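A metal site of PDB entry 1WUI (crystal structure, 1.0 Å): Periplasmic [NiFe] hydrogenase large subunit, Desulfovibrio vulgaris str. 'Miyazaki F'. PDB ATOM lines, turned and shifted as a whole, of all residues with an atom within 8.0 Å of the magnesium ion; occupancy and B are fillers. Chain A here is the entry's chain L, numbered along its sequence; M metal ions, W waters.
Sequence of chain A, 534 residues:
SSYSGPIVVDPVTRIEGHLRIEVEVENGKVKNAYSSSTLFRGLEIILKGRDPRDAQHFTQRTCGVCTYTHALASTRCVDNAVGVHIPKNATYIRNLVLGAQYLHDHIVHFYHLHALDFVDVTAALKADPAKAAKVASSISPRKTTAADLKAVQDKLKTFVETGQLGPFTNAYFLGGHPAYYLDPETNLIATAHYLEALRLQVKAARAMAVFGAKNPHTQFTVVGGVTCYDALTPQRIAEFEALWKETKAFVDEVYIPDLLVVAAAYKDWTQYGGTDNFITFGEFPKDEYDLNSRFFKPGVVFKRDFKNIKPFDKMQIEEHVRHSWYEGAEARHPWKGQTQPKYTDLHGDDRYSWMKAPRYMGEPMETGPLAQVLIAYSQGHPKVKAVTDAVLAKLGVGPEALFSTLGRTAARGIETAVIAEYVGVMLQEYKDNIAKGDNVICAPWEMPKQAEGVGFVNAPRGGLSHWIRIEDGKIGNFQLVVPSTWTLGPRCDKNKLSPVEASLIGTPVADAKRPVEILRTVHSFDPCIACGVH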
ATOM      1  N   PHE A  40      23.027  15.468  18.992  1.00  0.00           N
ATOM      2  CA  PHE A  40      23.709  16.498  18.259  1.00  0.00           C
ATOM      3  C   PHE A  40      24.828  15.883  17.443  1.00  0.00           C
ATOM      4  O   PHE A  40      25.530  14.983  17.947  1.00  0.00           O
ATOM      5  CB  PHE A  40      24.265  17.511  19.242  1.00  0.00           C
ATOM      6  CG  PHE A  40      25.103  18.610  18.633  1.00  0.00           C
ATOM      7  CD1 PHE A  40      24.508  19.704  18.042  1.00  0.00           C
ATOM      8  CD2 PHE A  40      26.502  18.555  18.675  1.00  0.00           C
ATOM      9  CE1 PHE A  40      25.251  20.732  17.476  1.00  0.00           C
ATOM     10  CE2 PHE A  40      27.241  19.570  18.140  1.00  0.00           C
ATOM     11  CZ  PHE A  40      26.652  20.660  17.561  1.00  0.00           C
ATOM     12  N   GLU A  44      27.408  21.918  11.035  1.00  0.00           N
ATOM     13  CA  GLU A  44      27.827  23.315  10.779  1.00  0.00           C
ATOM     14  C   GLU A  44      29.253  23.577  11.231  1.00  0.00           C
ATOM     15  O   GLU A  44      29.999  24.286  10.563  1.00  0.00           O
ATOM     16  CB  GLU A  44      26.870  24.291  11.419  1.00  0.00           C
ATOM     17  CG  GLU A  44      25.445  24.235  10.844  1.00  0.00           C
ATOM     18  CD  GLU A  44      24.361  24.668  11.791  1.00  0.00           C
ATOM     19  OE1 GLU A  44      24.594  24.581  13.019  1.00  0.00           O
ATOM     20  OE2 GLU A  44      23.268  25.027  11.317  1.00  0.00           O
ATOM     21  N   GLU A 319      17.530  32.553  15.168  1.00  0.00           N
ATOM     22  CA  GLU A 319      17.511  31.292  15.894  1.00  0.00           C
ATOM     23  C   GLU A 319      17.985  31.510  17.318  1.00  0.00           C
ATOM     24  O   GLU A 319      19.116  31.937  17.568  1.00  0.00           O
ATOM     25  CB  GLU A 319      18.403  30.237  15.223  1.00  0.00           C
ATOM     26  CG  GLU A 319      17.887  29.845  13.854  1.00  0.00           C
ATOM     27  CD  GLU A 319      18.719  28.716  13.325  1.00  0.00           C
ATOM     28  OE1 GLU A 319      18.234  27.569  13.333  1.00  0.00           O
ATOM     29  OE2 GLU A 319      19.880  28.981  12.914  1.00  0.00           O
ATOM     30  N   TYR A 326      23.343  25.360  23.912  1.00  0.00           N
ATOM     31  CA  TYR A 326      24.360  26.149  23.267  1.00  0.00           C
ATOM     32  C   TYR A 326      24.721  27.278  24.222  1.00  0.00           C
ATOM     33  O   TYR A 326      24.014  27.589  25.174  1.00  0.00           O
ATOM     34  CB  TYR A 326      23.945  26.739  21.890  1.00  0.00           C
ATOM     35  CG  TYR A 326      23.559  25.625  20.928  1.00  0.00           C
ATOM     36  CD1 TYR A 326      22.224  25.238  20.791  1.00  0.00           C
ATOM     37  CD2 TYR A 326      24.514  24.931  20.244  1.00  0.00           C
ATOM     38  CE1 TYR A 326      21.875  24.190  19.926  1.00  0.00           C
ATOM     39  CE2 TYR A 326      24.181  23.889  19.407  1.00  0.00           C
ATOM     40  CZ  TYR A 326      22.852  23.522  19.234  1.00  0.00           C
ATOM     41  OH  TYR A 326      22.564  22.460  18.433  1.00  0.00           O
ATOM     42  N   PRO A 334      20.839  33.662  10.592  1.00  0.00           N
ATOM     43  CA  PRO A 334      21.807  32.610  10.158  1.00  0.00           C
ATOM     44  C   PRO A 334      23.028  33.037   9.414  1.00  0.00           C
ATOM     45  O   PRO A 334      24.025  32.347   9.455  1.00  0.00           O
ATOM     46  CB  PRO A 334      20.945  31.645   9.340  1.00  0.00           C
ATOM     47  CG  PRO A 334      19.610  32.203   9.304  1.00  0.00           C
ATOM     48  CD  PRO A 334      19.484  33.390  10.151  1.00  0.00           C
ATOM     49  N   GLY A 337      25.166  33.236  12.221  1.00  0.00           N
ATOM     50  CA  GLY A 337      24.839  32.151  13.144  1.00  0.00           C
ATOM     51  C   GLY A 337      26.038  31.673  13.945  1.00  0.00           C
ATOM     52  O   GLY A 337      27.226  31.853  13.572  1.00  0.00           O
ATOM     53  N   GLN A 338      25.717  30.999  15.042  1.00  0.00           N
ATOM     54  CA  GLN A 338      26.686  30.412  15.938  1.00  0.00           C
ATOM     55  C   GLN A 338      26.245  29.029  16.367  1.00  0.00           C
ATOM     56  O   GLN A 338      25.053  28.881  16.655  1.00  0.00           O
ATOM     57  CB  GLN A 338      26.875  31.261  17.228  1.00  0.00           C
ATOM     58  CG  GLN A 338      27.355  32.660  16.919  1.00  0.00           C
ATOM     59  CD  GLN A 338      27.530  33.458  18.180  1.00  0.00           C
ATOM     60  OE1 GLN A 338      28.678  33.921  18.443  1.00  0.00           O
ATOM     61  NE2 GLN A 338      26.482  33.582  18.970  1.00  0.00           N
ATOM     62  N   THR A 339      27.167  28.090  16.403  1.00  0.00           N
ATOM     63  CA  THR A 339      26.839  26.721  16.824  1.00  0.00           C
ATOM     64  C   THR A 339      27.899  26.336  17.801  1.00  0.00           C
ATOM     65  O   THR A 339      28.938  25.788  17.437  1.00  0.00           O
ATOM     66  CB  THR A 339      26.719  25.783  15.625  1.00  0.00           C
ATOM     67  OG1 THR A 339      25.808  26.392  14.726  1.00  0.00           O
ATOM     68  CG2 THR A 339      26.249  24.404  16.095  1.00  0.00           C
ATOM     69  N   TRP A 354      18.796  19.987  21.891  1.00  0.00           N
ATOM     70  CA  TRP A 354      19.849  20.297  20.952  1.00  0.00           C
ATOM     71  C   TRP A 354      19.352  21.137  19.773  1.00  0.00           C
ATOM     72  O   TRP A 354      20.157  21.595  18.959  1.00  0.00           O
ATOM     73  CB  TRP A 354      20.557  19.064  20.437  1.00  0.00           C
ATOM     74  CG  TRP A 354      21.445  18.435  21.472  1.00  0.00           C
ATOM     75  CD1 TRP A 354      21.283  17.260  22.125  1.00  0.00           C
ATOM     76  CD2 TRP A 354      22.660  19.001  21.973  1.00  0.00           C
ATOM     77  NE1 TRP A 354      22.318  17.019  22.993  1.00  0.00           N
ATOM     78  CE2 TRP A 354      23.171  18.085  22.910  1.00  0.00           C
ATOM     79  CE3 TRP A 354      23.389  20.162  21.712  1.00  0.00           C
ATOM     80  CZ2 TRP A 354      24.368  18.338  23.610  1.00  0.00           C
ATOM     81  CZ3 TRP A 354      24.564  20.413  22.388  1.00  0.00           C
ATOM     82  CH2 TRP A 354      25.032  19.500  23.314  1.00  0.00           C
ATOM     83  N   MET A 355      18.035  21.291  19.563  1.00  0.00           N
ATOM     84  CA  MET A 355      17.579  22.158  18.531  1.00  0.00           C
ATOM     85  C   MET A 355      17.661  23.644  19.000  1.00  0.00           C
ATOM     86  O   MET A 355      17.321  23.918  20.134  1.00  0.00           O
ATOM     87  CB  MET A 355      16.144  21.918  18.100  1.00  0.00           C
ATOM     88  CG  MET A 355      15.946  20.652  17.305  1.00  0.00           C
ATOM     89  SD  MET A 355      14.321  20.675  16.525  1.00  0.00           S
ATOM     90  CE  MET A 355      14.022  18.944  16.145  1.00  0.00           C
ATOM     91  N   LYS A 356      18.058  24.505  18.084  1.00  0.00           N
ATOM     92  CA  LYS A 356      17.814  25.952  18.240  1.00  0.00           C
ATOM     93  C   LYS A 356      16.309  26.201  18.073  1.00  0.00           C
ATOM     94  O   LYS A 356      15.550  25.322  17.651  1.00  0.00           O
ATOM     95  CB  LYS A 356      18.613  26.718  17.245  1.00  0.00           C
ATOM     96  CG  LYS A 356      20.147  26.541  17.335  1.00  0.00           C
ATOM     97  CD  LYS A 356      20.878  27.296  16.260  1.00  0.00           C
ATOM     98  CE  LYS A 356      22.380  27.082  16.360  1.00  0.00           C
ATOM     99  NZ  LYS A 356      23.078  27.598  15.138  1.00  0.00           N
ATOM    100  N   PRO A 358      14.031  28.681  16.075  1.00  0.00           N
ATOM    101  CA  PRO A 358      13.870  29.718  15.080  1.00  0.00           C
ATOM    102  C   PRO A 358      12.581  30.469  15.342  1.00  0.00           C
ATOM    103  O   PRO A 358      11.535  29.893  15.666  1.00  0.00           O
ATOM    104  CB  PRO A 358      13.792  28.973  13.743  1.00  0.00           C
ATOM    105  CG  PRO A 358      14.309  27.600  14.053  1.00  0.00           C
ATOM    106  CD  PRO A 358      13.865  27.335  15.475  1.00  0.00           C
ATOM    107  N   SER A 465      16.254  26.276   4.751  1.00  0.00           N
ATOM    108  CA  SER A 465      17.179  27.276   4.228  1.00  0.00           C
ATOM    109  C   SER A 465      18.590  26.926   4.692  1.00  0.00           C
ATOM    110  O   SER A 465      18.824  26.541   5.827  1.00  0.00           O
ATOM    111  CB  SER A 465      16.747  28.699   4.615  1.00  0.00           C
ATOM    112  OG  SER A 465      16.576  28.891   6.000  1.00  0.00           O
ATOM    113  N   TRP A 467      22.521  28.668   4.502  1.00  0.00           N
ATOM    114  CA  TRP A 467      23.082  30.012   4.489  1.00  0.00           C
ATOM    115  C   TRP A 467      24.613  29.956   4.541  1.00  0.00           C
ATOM    116  O   TRP A 467      25.134  29.345   5.478  1.00  0.00           O
ATOM    117  CB  TRP A 467      22.581  30.775   5.707  1.00  0.00           C
ATOM    118  CG  TRP A 467      21.110  30.829   5.881  1.00  0.00           C
ATOM    119  CD1 TRP A 467      20.314  29.839   6.321  1.00  0.00           C
ATOM    120  CD2 TRP A 467      20.262  31.967   5.618  1.00  0.00           C
ATOM    121  NE1 TRP A 467      19.001  30.324   6.363  1.00  0.00           N
ATOM    122  CE2 TRP A 467      18.956  31.617   5.936  1.00  0.00           C
ATOM    123  CE3 TRP A 467      20.529  33.271   5.153  1.00  0.00           C
ATOM    124  CZ2 TRP A 467      17.868  32.480   5.811  1.00  0.00           C
ATOM    125  CZ3 TRP A 467      19.463  34.133   5.034  1.00  0.00           C
ATOM    126  CH2 TRP A 467      18.184  33.725   5.358  1.00  0.00           C
ATOM    127  N   PHE A 478      28.510  28.338   7.699  1.00  0.00           N
ATOM    128  CA  PHE A 478      27.451  27.630   7.004  1.00  0.00           C
ATOM    129  C   PHE A 478      26.432  27.268   8.048  1.00  0.00           C
ATOM    130  O   PHE A 478      26.744  26.592   9.029  1.00  0.00           O
ATOM    131  CB  PHE A 478      28.006  26.387   6.294  1.00  0.00           C
ATOM    132  CG  PHE A 478      27.097  25.920   5.169  1.00  0.00           C
ATOM    133  CD1 PHE A 478      25.898  25.290   5.431  1.00  0.00           C
ATOM    134  CD2 PHE A 478      27.480  26.160   3.866  1.00  0.00           C
ATOM    135  CE1 PHE A 478      25.086  24.886   4.391  1.00  0.00           C
ATOM    136  CE2 PHE A 478      26.661  25.761   2.814  1.00  0.00           C
ATOM    137  CZ  PHE A 478      25.424  25.152   3.085  1.00  0.00           C
ATOM    138  N   GLN A 479      25.200  27.732   7.853  1.00  0.00           N
ATOM    139  CA  GLN A 479      24.114  27.518   8.811  1.00  0.00           C
ATOM    140  C   GLN A 479      22.921  26.906   8.100  1.00  0.00           C
ATOM    141  O   GLN A 479      22.497  27.382   7.049  1.00  0.00           O
ATOM    142  CB  GLN A 479      23.761  28.826   9.489  1.00  0.00           C
ATOM    143  CG  GLN A 479      24.871  29.391  10.363  1.00  0.00           C
ATOM    144  CD  GLN A 479      25.088  28.635  11.633  1.00  0.00           C
ATOM    145  OE1 GLN A 479      24.154  28.091  12.237  1.00  0.00           O
ATOM    146  NE2 GLN A 479      26.333  28.591  12.134  1.00  0.00           N
ATOM    147  N   LEU A 480      22.422  25.837   8.715  1.00  0.00           N
ATOM    148  CA  LEU A 480      21.186  25.200   8.280  1.00  0.00           C
ATOM    149  C   LEU A 480      20.068  25.617   9.230  1.00  0.00           C
ATOM    150  O   LEU A 480      20.233  25.546  10.439  1.00  0.00           O
ATOM    151  CB  LEU A 480      21.252  23.682   8.291  1.00  0.00           C
ATOM    152  CG  LEU A 480      22.321  23.038   7.397  1.00  0.00           C
ATOM    153  CD1 LEU A 480      23.717  23.159   7.779  1.00  0.00           C
ATOM    154  CD2 LEU A 480      21.961  21.508   7.320  1.00  0.00           C
ATOM    155  N   VAL A 481      18.936  26.016   8.682  1.00  0.00           N
ATOM    156  CA  VAL A 481      17.710  26.319   9.459  1.00  0.00           C
ATOM    157  C   VAL A 481      16.657  25.422   8.832  1.00  0.00           C
ATOM    158  O   VAL A 481      16.320  25.593   7.676  1.00  0.00           O
ATOM    159  CB  VAL A 481      17.297  27.774   9.435  1.00  0.00           C
ATOM    160  CG1 VAL A 481      16.146  27.996  10.418  1.00  0.00           C
ATOM    161  CG2 VAL A 481      18.469  28.678   9.775  1.00  0.00           C
ATOM    162  N   VAL A 482      16.222  24.382   9.559  1.00  0.00           N
ATOM    163  CA  VAL A 482      15.525  23.259   8.909  1.00  0.00           C
ATOM    164  C   VAL A 482      14.084  23.233   9.353  1.00  0.00           C
ATOM    165  O   VAL A 482      13.742  23.738  10.449  1.00  0.00           O
ATOM    166  CB  VAL A 482      16.337  21.976   9.276  1.00  0.00           C
ATOM    167  CG1 VAL A 482      15.892  20.753   8.583  1.00  0.00           C
ATOM    168  CG2 VAL A 482      17.815  22.196   8.901  1.00  0.00           C
ATOM    169  N   THR A 485      13.348  22.209  12.812  1.00  0.00           N
ATOM    170  CA  THR A 485      13.855  23.178  13.778  1.00  0.00           C
ATOM    171  C   THR A 485      12.752  24.183  14.102  1.00  0.00           C
ATOM    172  O   THR A 485      12.502  24.492  15.272  1.00  0.00           O
ATOM    173  CB  THR A 485      15.121  23.919  13.236  1.00  0.00           C
ATOM    174  OG1 THR A 485      15.959  23.060  12.473  1.00  0.00           O
ATOM    175  CG2 THR A 485      15.875  24.521  14.410  1.00  0.00           C
ATOM    176  N   CYS A 531      17.392  16.244  10.958  1.00  0.00           N
ATOM    177  CA  CYS A 531      17.135  17.525  10.331  1.00  0.00           C
ATOM    178  C   CYS A 531      17.133  18.643  11.325  1.00  0.00           C
ATOM    179  O   CYS A 531      17.824  19.696  11.100  1.00  0.00           O
ATOM    180  CB  CYS A 531      15.752  17.498   9.590  1.00  0.00           C
ATOM    181  SG  CYS A 531      15.915  16.962   7.906  1.00  0.00           S
ATOM    182  N   GLY A 532      16.370  18.570  12.385  1.00  0.00           N
ATOM    183  CA  GLY A 532      16.201  19.734  13.195  1.00  0.00           C
ATOM    184  C   GLY A 532      17.479  20.197  13.875  1.00  0.00           C
ATOM    185  O   GLY A 532      17.626  21.391  14.080  1.00  0.00           O
ATOM    186  N   VAL A 533      18.324  19.251  14.285  1.00  0.00           N
ATOM    187  CA  VAL A 533      19.540  19.548  15.008  1.00  0.00           C
ATOM    188  C   VAL A 533      20.785  19.652  14.149  1.00  0.00           C
ATOM    189  O   VAL A 533      21.636  20.550  14.336  1.00  0.00           O
ATOM    190  CB  VAL A 533      19.831  18.510  16.089  1.00  0.00           C
ATOM    191  CG1 VAL A 533      21.127  18.832  16.850  1.00  0.00           C
ATOM    192  CG2 VAL A 533      18.670  18.347  17.076  1.00  0.00           C
ATOM    193  N   HIS A 534      20.974  18.714  13.215  1.00  0.00           N
ATOM    194  CA  HIS A 534      22.169  18.640  12.389  1.00  0.00           C
ATOM    195  C   HIS A 534      23.462  18.774  13.246  1.00  0.00           C
ATOM    196  O   HIS A 534      23.485  18.071  14.332  1.00  0.00           O
ATOM    197  CB  HIS A 534      22.121  19.561  11.139  1.00  0.00           C
ATOM    198  CG  HIS A 534      21.564  20.942  11.380  1.00  0.00           C
ATOM    199  ND1 HIS A 534      20.214  21.135  11.473  1.00  0.00           N
ATOM    200  CD2 HIS A 534      22.101  22.122  11.665  1.00  0.00           C
ATOM    201  CE1 HIS A 534      19.981  22.423  11.764  1.00  0.00           C
ATOM    202  NE2 HIS A 534      21.128  23.084  11.894  1.00  0.00           N
ATOM    203  OXT HIS A 534      24.399  19.480  12.832  1.00  0.00           O
HETATM  204 MG    MG M   1      21.318  25.163  12.224  1.00  0.00          MG
HETATM  205  O   HOH W   1      19.473  25.258  13.181  1.00  0.00           O
HETATM  206  O   HOH W   2      21.672  27.163  12.445  1.00  0.00           O
HETATM  207  O   HOH W   3      22.231  24.857  14.111  1.00  0.00           O
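Water W3 bridges OE1 of Glu 44 (2.6 Å) and NZ of Lys 356 (3.0 Å). Water W2 lies within hydrogen-bond range of the side-chain carboxylate (OE2) of Glu 319 (2.6 Å), the side-chain amide oxygen (OE1) of Gln 479 (2.7 Å) and the side-chain amino group (NZ) of Lys 356 (3.1 Å).
Three residues have an atom within 4 Å of the magnesium ion: Glu 44, Leu 480 and His 534.
The backbone carbonyl oxygen of Cys 531 sits at hydrogen-bond distance from a ring nitrogen (ND1) of His 534, 2.8 Å away. The side-chain carboxylate (OE2) of Glu 44 lies close to the side-chain amide oxygen (OE1) of Gln 479, at 3.3 Å. NZ of Lys 356 is in salt-bridge range of OE1 of Glu 44, 3.99 Å away. OE1 of Glu 44 is in hydrogen-bond range of OG1 of Thr 339 (2.8 Å).
Water W2 binds the magnesium ion, at 2.0 Å. Water W1 binds the magnesium ion (2.1 Å). NE2 of His 534 is bound to the magnesium ion (2.1 Å). Water W3 binds the magnesium ion (2.1 Å). O of Leu 480 binds the magnesium ion (2.1 Å). OE2 of Glu 44 is bound to the magnesium ion. The magnesium ion has six donor atoms within binding distance.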
